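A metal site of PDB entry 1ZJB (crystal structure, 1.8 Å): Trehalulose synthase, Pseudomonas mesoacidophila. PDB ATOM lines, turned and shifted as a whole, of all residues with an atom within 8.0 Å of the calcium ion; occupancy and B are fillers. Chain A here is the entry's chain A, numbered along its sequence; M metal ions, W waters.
The calcium ion is bound by OD1 of Asp 22, at 2.3 Å. The calcium ion is bound by OD2 of Asp 30 (2.3 Å). The calcium ion is bound by OD1 of Asn 24, at 2.3 Å. The calcium ion is bound by water W1, 2.4 Å away. O of Ile 28 binds the calcium ion. OD1 of Asp 26 is bound to the calcium ion. The calcium ion is bound by water W2 (2.4 Å).
Water W2 bridges the side-chain amide nitrogen (ND2) of Asn 24 (3.2 Å) and the backbone carbonyl oxygen (O) of Glu 75 (3.2 Å). Water W1 bridges the backbone carbonyl oxygen (O) of Glu 75 and the side-chain carboxylate (OD2) of Asp 26.
N of Asp 22 sits at hydrogen-bond distance from O of Phe 431 (3.0 Å). The side-chain carboxylate (OD2) of Asp 22 sits at hydrogen-bond distance from the backbone NH (N) of Gly 27, 2.8 Å away. The backbone NH (N) of Gly 25 sits at hydrogen-bond distance from the side-chain carboxylate (OD2) of Asp 22, 3.3 Å away. The side-chain carboxylate (OD1) of Asp 30 sits at hydrogen-bond distance from the side-chain hydroxyl (OG1) of Thr 23, 2.6 Å away. The side-chain carboxylate of Asp 22 lies within hydrogen-bond range of the side-chain hydroxyl of Thr 432, at 2.7 Å. The backbone NH (N) of Asp 30 lies within hydrogen-bond range of the backbone carbonyl oxygen (O) of Lys 21 (3.0 Å). OD1 of Asp 30 lies within hydrogen-bond range of N of Gly 33.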
ATOM      1  N   PRO A  17     -17.829  20.292 -13.763  1.00  0.00           N
ATOM      2  CA  PRO A  17     -17.820  21.757 -13.580  1.00  0.00           C
ATOM      3  C   PRO A  17     -16.493  22.395 -13.213  1.00  0.00           C
ATOM      4  O   PRO A  17     -16.106  23.398 -13.803  1.00  0.00           O
ATOM      5  CB  PRO A  17     -18.877  21.991 -12.503  1.00  0.00           C
ATOM      6  CG  PRO A  17     -19.800  20.815 -12.677  1.00  0.00           C
ATOM      7  CD  PRO A  17     -18.820  19.685 -12.858  1.00  0.00           C
ATOM      8  N   ARG A  18     -15.811  21.797 -12.238  1.00  0.00           N
ATOM      9  CA  ARG A  18     -14.531  22.307 -11.769  1.00  0.00           C
ATOM     10  C   ARG A  18     -13.537  22.558 -12.915  1.00  0.00           C
ATOM     11  O   ARG A  18     -12.683  23.438 -12.827  1.00  0.00           O
ATOM     12  CB  ARG A  18     -13.950  21.269 -10.796  1.00  0.00           C
ATOM     13  CG  ARG A  18     -12.764  21.737 -10.013  1.00  0.00           C
ATOM     14  CD  ARG A  18     -12.310  20.648  -9.054  1.00  0.00           C
ATOM     15  NE  ARG A  18     -11.161  21.100  -8.290  1.00  0.00           N
ATOM     16  CZ  ARG A  18     -11.229  21.813  -7.177  1.00  0.00           C
ATOM     17  NH1 ARG A  18     -12.400  22.143  -6.655  1.00  0.00           N
ATOM     18  NH2 ARG A  18     -10.105  22.218  -6.586  1.00  0.00           N
ATOM     19  N   LYS A  21     -15.473  25.455 -17.447  1.00  0.00           N
ATOM     20  CA  LYS A  21     -15.256  26.877 -17.807  1.00  0.00           C
ATOM     21  C   LYS A  21     -15.298  27.830 -16.608  1.00  0.00           C
ATOM     22  O   LYS A  21     -16.311  27.932 -15.907  1.00  0.00           O
ATOM     23  CB  LYS A  21     -16.270  27.335 -18.853  1.00  0.00           C
ATOM     24  CG  LYS A  21     -16.103  28.812 -19.329  1.00  0.00           C
ATOM     25  CD  LYS A  21     -14.727  29.073 -19.931  1.00  0.00           C
ATOM     26  CE  LYS A  21     -14.657  30.401 -20.722  1.00  0.00           C
ATOM     27  NZ  LYS A  21     -15.274  31.512 -19.990  1.00  0.00           N
ATOM     28  N   ASP A  22     -14.171  28.522 -16.375  1.00  0.00           N
ATOM     29  CA  ASP A  22     -14.041  29.491 -15.273  1.00  0.00           C
ATOM     30  C   ASP A  22     -14.418  30.864 -15.803  1.00  0.00           C
ATOM     31  O   ASP A  22     -13.947  31.275 -16.865  1.00  0.00           O
ATOM     32  CB  ASP A  22     -12.587  29.528 -14.781  1.00  0.00           C
ATOM     33  CG  ASP A  22     -12.372  30.528 -13.631  1.00  0.00           C
ATOM     34  OD1 ASP A  22     -13.357  30.958 -12.997  1.00  0.00           O
ATOM     35  OD2 ASP A  22     -11.210  30.861 -13.361  1.00  0.00           O
ATOM     36  N   THR A  23     -15.269  31.578 -15.070  1.00  0.00           N
ATOM     37  CA  THR A  23     -15.680  32.913 -15.530  1.00  0.00           C
ATOM     38  C   THR A  23     -15.320  34.016 -14.542  1.00  0.00           C
ATOM     39  O   THR A  23     -15.795  35.139 -14.684  1.00  0.00           O
ATOM     40  CB  THR A  23     -17.203  33.001 -15.741  1.00  0.00           C
ATOM     41  OG1 THR A  23     -17.875  32.614 -14.540  1.00  0.00           O
ATOM     42  CG2 THR A  23     -17.636  32.114 -16.900  1.00  0.00           C
ATOM     43  N   ASN A  24     -14.511  33.733 -13.535  1.00  0.00           N
ATOM     44  CA  ASN A  24     -14.155  34.775 -12.601  1.00  0.00           C
ATOM     45  C   ASN A  24     -12.689  34.755 -12.218  1.00  0.00           C
ATOM     46  O   ASN A  24     -12.289  35.368 -11.244  1.00  0.00           O
ATOM     47  CB  ASN A  24     -15.072  34.722 -11.365  1.00  0.00           C
ATOM     48  CG  ASN A  24     -14.720  33.603 -10.436  1.00  0.00           C
ATOM     49  OD1 ASN A  24     -14.185  32.569 -10.858  1.00  0.00           O
ATOM     50  ND2 ASN A  24     -15.020  33.775  -9.151  1.00  0.00           N
ATOM     51  N   GLY A  25     -11.888  34.025 -12.981  1.00  0.00           N
ATOM     52  CA  GLY A  25     -10.446  33.980 -12.766  1.00  0.00           C
ATOM     53  C   GLY A  25      -9.840  33.350 -11.527  1.00  0.00           C
ATOM     54  O   GLY A  25      -8.681  33.621 -11.229  1.00  0.00           O
ATOM     55  N   ASP A  26     -10.594  32.511 -10.808  1.00  0.00           N
ATOM     56  CA  ASP A  26     -10.015  31.876  -9.634  1.00  0.00           C
ATOM     57  C   ASP A  26      -9.398  30.535  -9.999  1.00  0.00           C
ATOM     58  O   ASP A  26      -8.861  29.829  -9.139  1.00  0.00           O
ATOM     59  CB  ASP A  26     -11.060  31.722  -8.526  1.00  0.00           C
ATOM     60  CG  ASP A  26     -12.187  30.751  -8.901  1.00  0.00           C
ATOM     61  OD1 ASP A  26     -12.392  30.450 -10.095  1.00  0.00           O
ATOM     62  OD2 ASP A  26     -12.889  30.317  -7.967  1.00  0.00           O
ATOM     63  N   GLY A  27      -9.443  30.184 -11.289  1.00  0.00           N
ATOM     64  CA  GLY A  27      -8.851  28.935 -11.756  1.00  0.00           C
ATOM     65  C   GLY A  27      -9.746  27.694 -11.625  1.00  0.00           C
ATOM     66  O   GLY A  27      -9.296  26.579 -11.894  1.00  0.00           O
ATOM     67  N   ILE A  28     -10.991  27.903 -11.221  1.00  0.00           N
ATOM     68  CA  ILE A  28     -11.947  26.806 -11.054  1.00  0.00           C
ATOM     69  C   ILE A  28     -13.199  27.072 -11.899  1.00  0.00           C
ATOM     70  O   ILE A  28     -13.706  28.196 -11.923  1.00  0.00           O
ATOM     71  CB  ILE A  28     -12.343  26.644  -9.567  1.00  0.00           C
ATOM     72  CG1 ILE A  28     -11.096  26.328  -8.740  1.00  0.00           C
ATOM     73  CG2 ILE A  28     -13.395  25.540  -9.411  1.00  0.00           C
ATOM     74  CD1 ILE A  28     -11.295  26.501  -7.233  1.00  0.00           C
ATOM     75  N   GLY A  29     -13.669  26.045 -12.599  1.00  0.00           N
ATOM     76  CA  GLY A  29     -14.858  26.177 -13.429  1.00  0.00           C
ATOM     77  C   GLY A  29     -16.075  26.459 -12.570  1.00  0.00           C
ATOM     78  O   GLY A  29     -16.086  26.150 -11.380  1.00  0.00           O
ATOM     79  N   ASP A  30     -17.112  27.032 -13.163  1.00  0.00           N
ATOM     80  CA  ASP A  30     -18.274  27.374 -12.373  1.00  0.00           C
ATOM     81  C   ASP A  30     -19.566  27.308 -13.192  1.00  0.00           C
ATOM     82  O   ASP A  30     -19.518  27.069 -14.405  1.00  0.00           O
ATOM     83  CB  ASP A  30     -18.076  28.782 -11.782  1.00  0.00           C
ATOM     84  CG  ASP A  30     -17.502  29.785 -12.802  1.00  0.00           C
ATOM     85  OD1 ASP A  30     -18.192  30.105 -13.792  1.00  0.00           O
ATOM     86  OD2 ASP A  30     -16.348  30.240 -12.611  1.00  0.00           O
ATOM     87  N   PHE A  31     -20.703  27.513 -12.531  1.00  0.00           N
ATOM     88  CA  PHE A  31     -21.998  27.457 -13.204  1.00  0.00           C
ATOM     89  C   PHE A  31     -22.146  28.471 -14.334  1.00  0.00           C
ATOM     90  O   PHE A  31     -22.708  28.150 -15.387  1.00  0.00           O
ATOM     91  CB  PHE A  31     -23.153  27.719 -12.227  1.00  0.00           C
ATOM     92  CG  PHE A  31     -23.346  26.639 -11.207  1.00  0.00           C
ATOM     93  CD1 PHE A  31     -23.410  25.311 -11.568  1.00  0.00           C
ATOM     94  CD2 PHE A  31     -23.538  26.971  -9.875  1.00  0.00           C
ATOM     95  CE1 PHE A  31     -23.673  24.311 -10.624  1.00  0.00           C
ATOM     96  CE2 PHE A  31     -23.799  26.007  -8.925  1.00  0.00           C
ATOM     97  CZ  PHE A  31     -23.866  24.663  -9.299  1.00  0.00           C
ATOM     98  N   LYS A  32     -21.698  29.698 -14.119  1.00  0.00           N
ATOM     99  CA  LYS A  32     -21.824  30.718 -15.167  1.00  0.00           C
ATOM    100  C   LYS A  32     -21.047  30.276 -16.391  1.00  0.00           C
ATOM    101  O   LYS A  32     -21.469  30.516 -17.535  1.00  0.00           O
ATOM    102  CB  LYS A  32     -21.297  32.080 -14.660  1.00  0.00           C
ATOM    103  CG  LYS A  32     -22.220  32.748 -13.648  1.00  0.00           C
ATOM    104  CD  LYS A  32     -21.627  34.054 -13.125  1.00  0.00           C
ATOM    105  CE  LYS A  32     -22.552  34.716 -12.119  1.00  0.00           C
ATOM    106  NZ  LYS A  32     -21.951  36.000 -11.604  1.00  0.00           N
ATOM    107  N   GLY A  33     -19.920  29.614 -16.160  1.00  0.00           N
ATOM    108  CA  GLY A  33     -19.124  29.122 -17.268  1.00  0.00           C
ATOM    109  C   GLY A  33     -19.884  28.075 -18.050  1.00  0.00           C
ATOM    110  O   GLY A  33     -19.899  28.083 -19.286  1.00  0.00           O
ATOM    111  N   LYS A  74     -19.770  26.625  -3.019  1.00  0.00           N
ATOM    112  CA  LYS A  74     -19.341  28.029  -3.119  1.00  0.00           C
ATOM    113  C   LYS A  74     -18.541  28.343  -4.379  1.00  0.00           C
ATOM    114  O   LYS A  74     -18.753  29.390  -5.010  1.00  0.00           O
ATOM    115  CB  LYS A  74     -18.538  28.419  -1.900  1.00  0.00           C
ATOM    116  CG  LYS A  74     -19.327  28.264  -0.610  1.00  0.00           C
ATOM    117  CD  LYS A  74     -18.574  28.863   0.565  1.00  0.00           C
ATOM    118  CE  LYS A  74     -18.363  30.368   0.376  1.00  0.00           C
ATOM    119  NZ  LYS A  74     -19.668  31.107   0.246  1.00  0.00           N
ATOM    120  N   GLU A  75     -17.625  27.456  -4.736  1.00  0.00           N
ATOM    121  CA  GLU A  75     -16.829  27.688  -5.930  1.00  0.00           C
ATOM    122  C   GLU A  75     -17.635  27.747  -7.224  1.00  0.00           C
ATOM    123  O   GLU A  75     -17.203  28.378  -8.173  1.00  0.00           O
ATOM    124  CB  GLU A  75     -15.770  26.596  -6.084  1.00  0.00           C
ATOM    125  CG  GLU A  75     -14.589  26.734  -5.145  1.00  0.00           C
ATOM    126  CD  GLU A  75     -14.857  26.160  -3.774  1.00  0.00           C
ATOM    127  OE1 GLU A  75     -15.994  25.701  -3.508  1.00  0.00           O
ATOM    128  OE2 GLU A  75     -13.926  26.162  -2.950  1.00  0.00           O
ATOM    129  N   TYR A  76     -18.778  27.074  -7.285  1.00  0.00           N
ATOM    130  CA  TYR A  76     -19.533  27.100  -8.539  1.00  0.00           C
ATOM    131  C   TYR A  76     -20.480  28.258  -8.668  1.00  0.00           C
ATOM    132  O   TYR A  76     -20.907  28.587  -9.758  1.00  0.00           O
ATOM    133  CB  TYR A  76     -20.300  25.794  -8.745  1.00  0.00           C
ATOM    134  CG  TYR A  76     -19.406  24.570  -8.853  1.00  0.00           C
ATOM    135  CD1 TYR A  76     -18.032  24.687  -9.063  1.00  0.00           C
ATOM    136  CD2 TYR A  76     -19.933  23.289  -8.699  1.00  0.00           C
ATOM    137  CE1 TYR A  76     -17.192  23.552  -9.105  1.00  0.00           C
ATOM    138  CE2 TYR A  76     -19.116  22.168  -8.750  1.00  0.00           C
ATOM    139  CZ  TYR A  76     -17.758  22.300  -8.943  1.00  0.00           C
ATOM    140  OH  TYR A  76     -16.957  21.176  -8.938  1.00  0.00           O
ATOM    141  N   GLY A  77     -20.807  28.886  -7.555  1.00  0.00           N
ATOM    142  CA  GLY A  77     -21.707  30.020  -7.622  1.00  0.00           C
ATOM    143  C   GLY A  77     -22.744  29.971  -6.530  1.00  0.00           C
ATOM    144  O   GLY A  77     -22.480  29.480  -5.423  1.00  0.00           O
ATOM    145  N   PHE A 431      -9.629  28.540 -20.767  1.00  0.00           N
ATOM    146  CA  PHE A 431     -10.422  27.996 -19.662  1.00  0.00           C
ATOM    147  C   PHE A 431     -10.532  29.023 -18.531  1.00  0.00           C
ATOM    148  O   PHE A 431     -11.589  29.135 -17.877  1.00  0.00           O
ATOM    149  CB  PHE A 431      -9.766  26.708 -19.139  1.00  0.00           C
ATOM    150  CG  PHE A 431     -10.216  26.305 -17.760  1.00  0.00           C
ATOM    151  CD1 PHE A 431     -11.502  25.820 -17.548  1.00  0.00           C
ATOM    152  CD2 PHE A 431      -9.356  26.438 -16.663  1.00  0.00           C
ATOM    153  CE1 PHE A 431     -11.931  25.482 -16.253  1.00  0.00           C
ATOM    154  CE2 PHE A 431      -9.775  26.100 -15.370  1.00  0.00           C
ATOM    155  CZ  PHE A 431     -11.065  25.614 -15.172  1.00  0.00           C
ATOM    156  N   THR A 432      -9.471  29.784 -18.314  1.00  0.00           N
ATOM    157  CA  THR A 432      -9.460  30.758 -17.233  1.00  0.00           C
ATOM    158  C   THR A 432      -8.493  31.901 -17.553  1.00  0.00           C
ATOM    159  O   THR A 432      -7.586  31.733 -18.382  1.00  0.00           O
ATOM    160  CB  THR A 432      -8.986  30.112 -15.907  1.00  0.00           C
ATOM    161  OG1 THR A 432      -9.010  31.078 -14.838  1.00  0.00           O
ATOM    162  CG2 THR A 432      -7.565  29.567 -16.055  1.00  0.00           C
HETATM  163 CA    CA M   1     -14.553  30.274 -11.138  1.00  0.00          CA
HETATM  164  O   HOH W   1     -14.946  28.885  -9.253  1.00  0.00           O
HETATM  165  O   HOH W   2     -16.443  31.038  -9.840  1.00  0.00           O
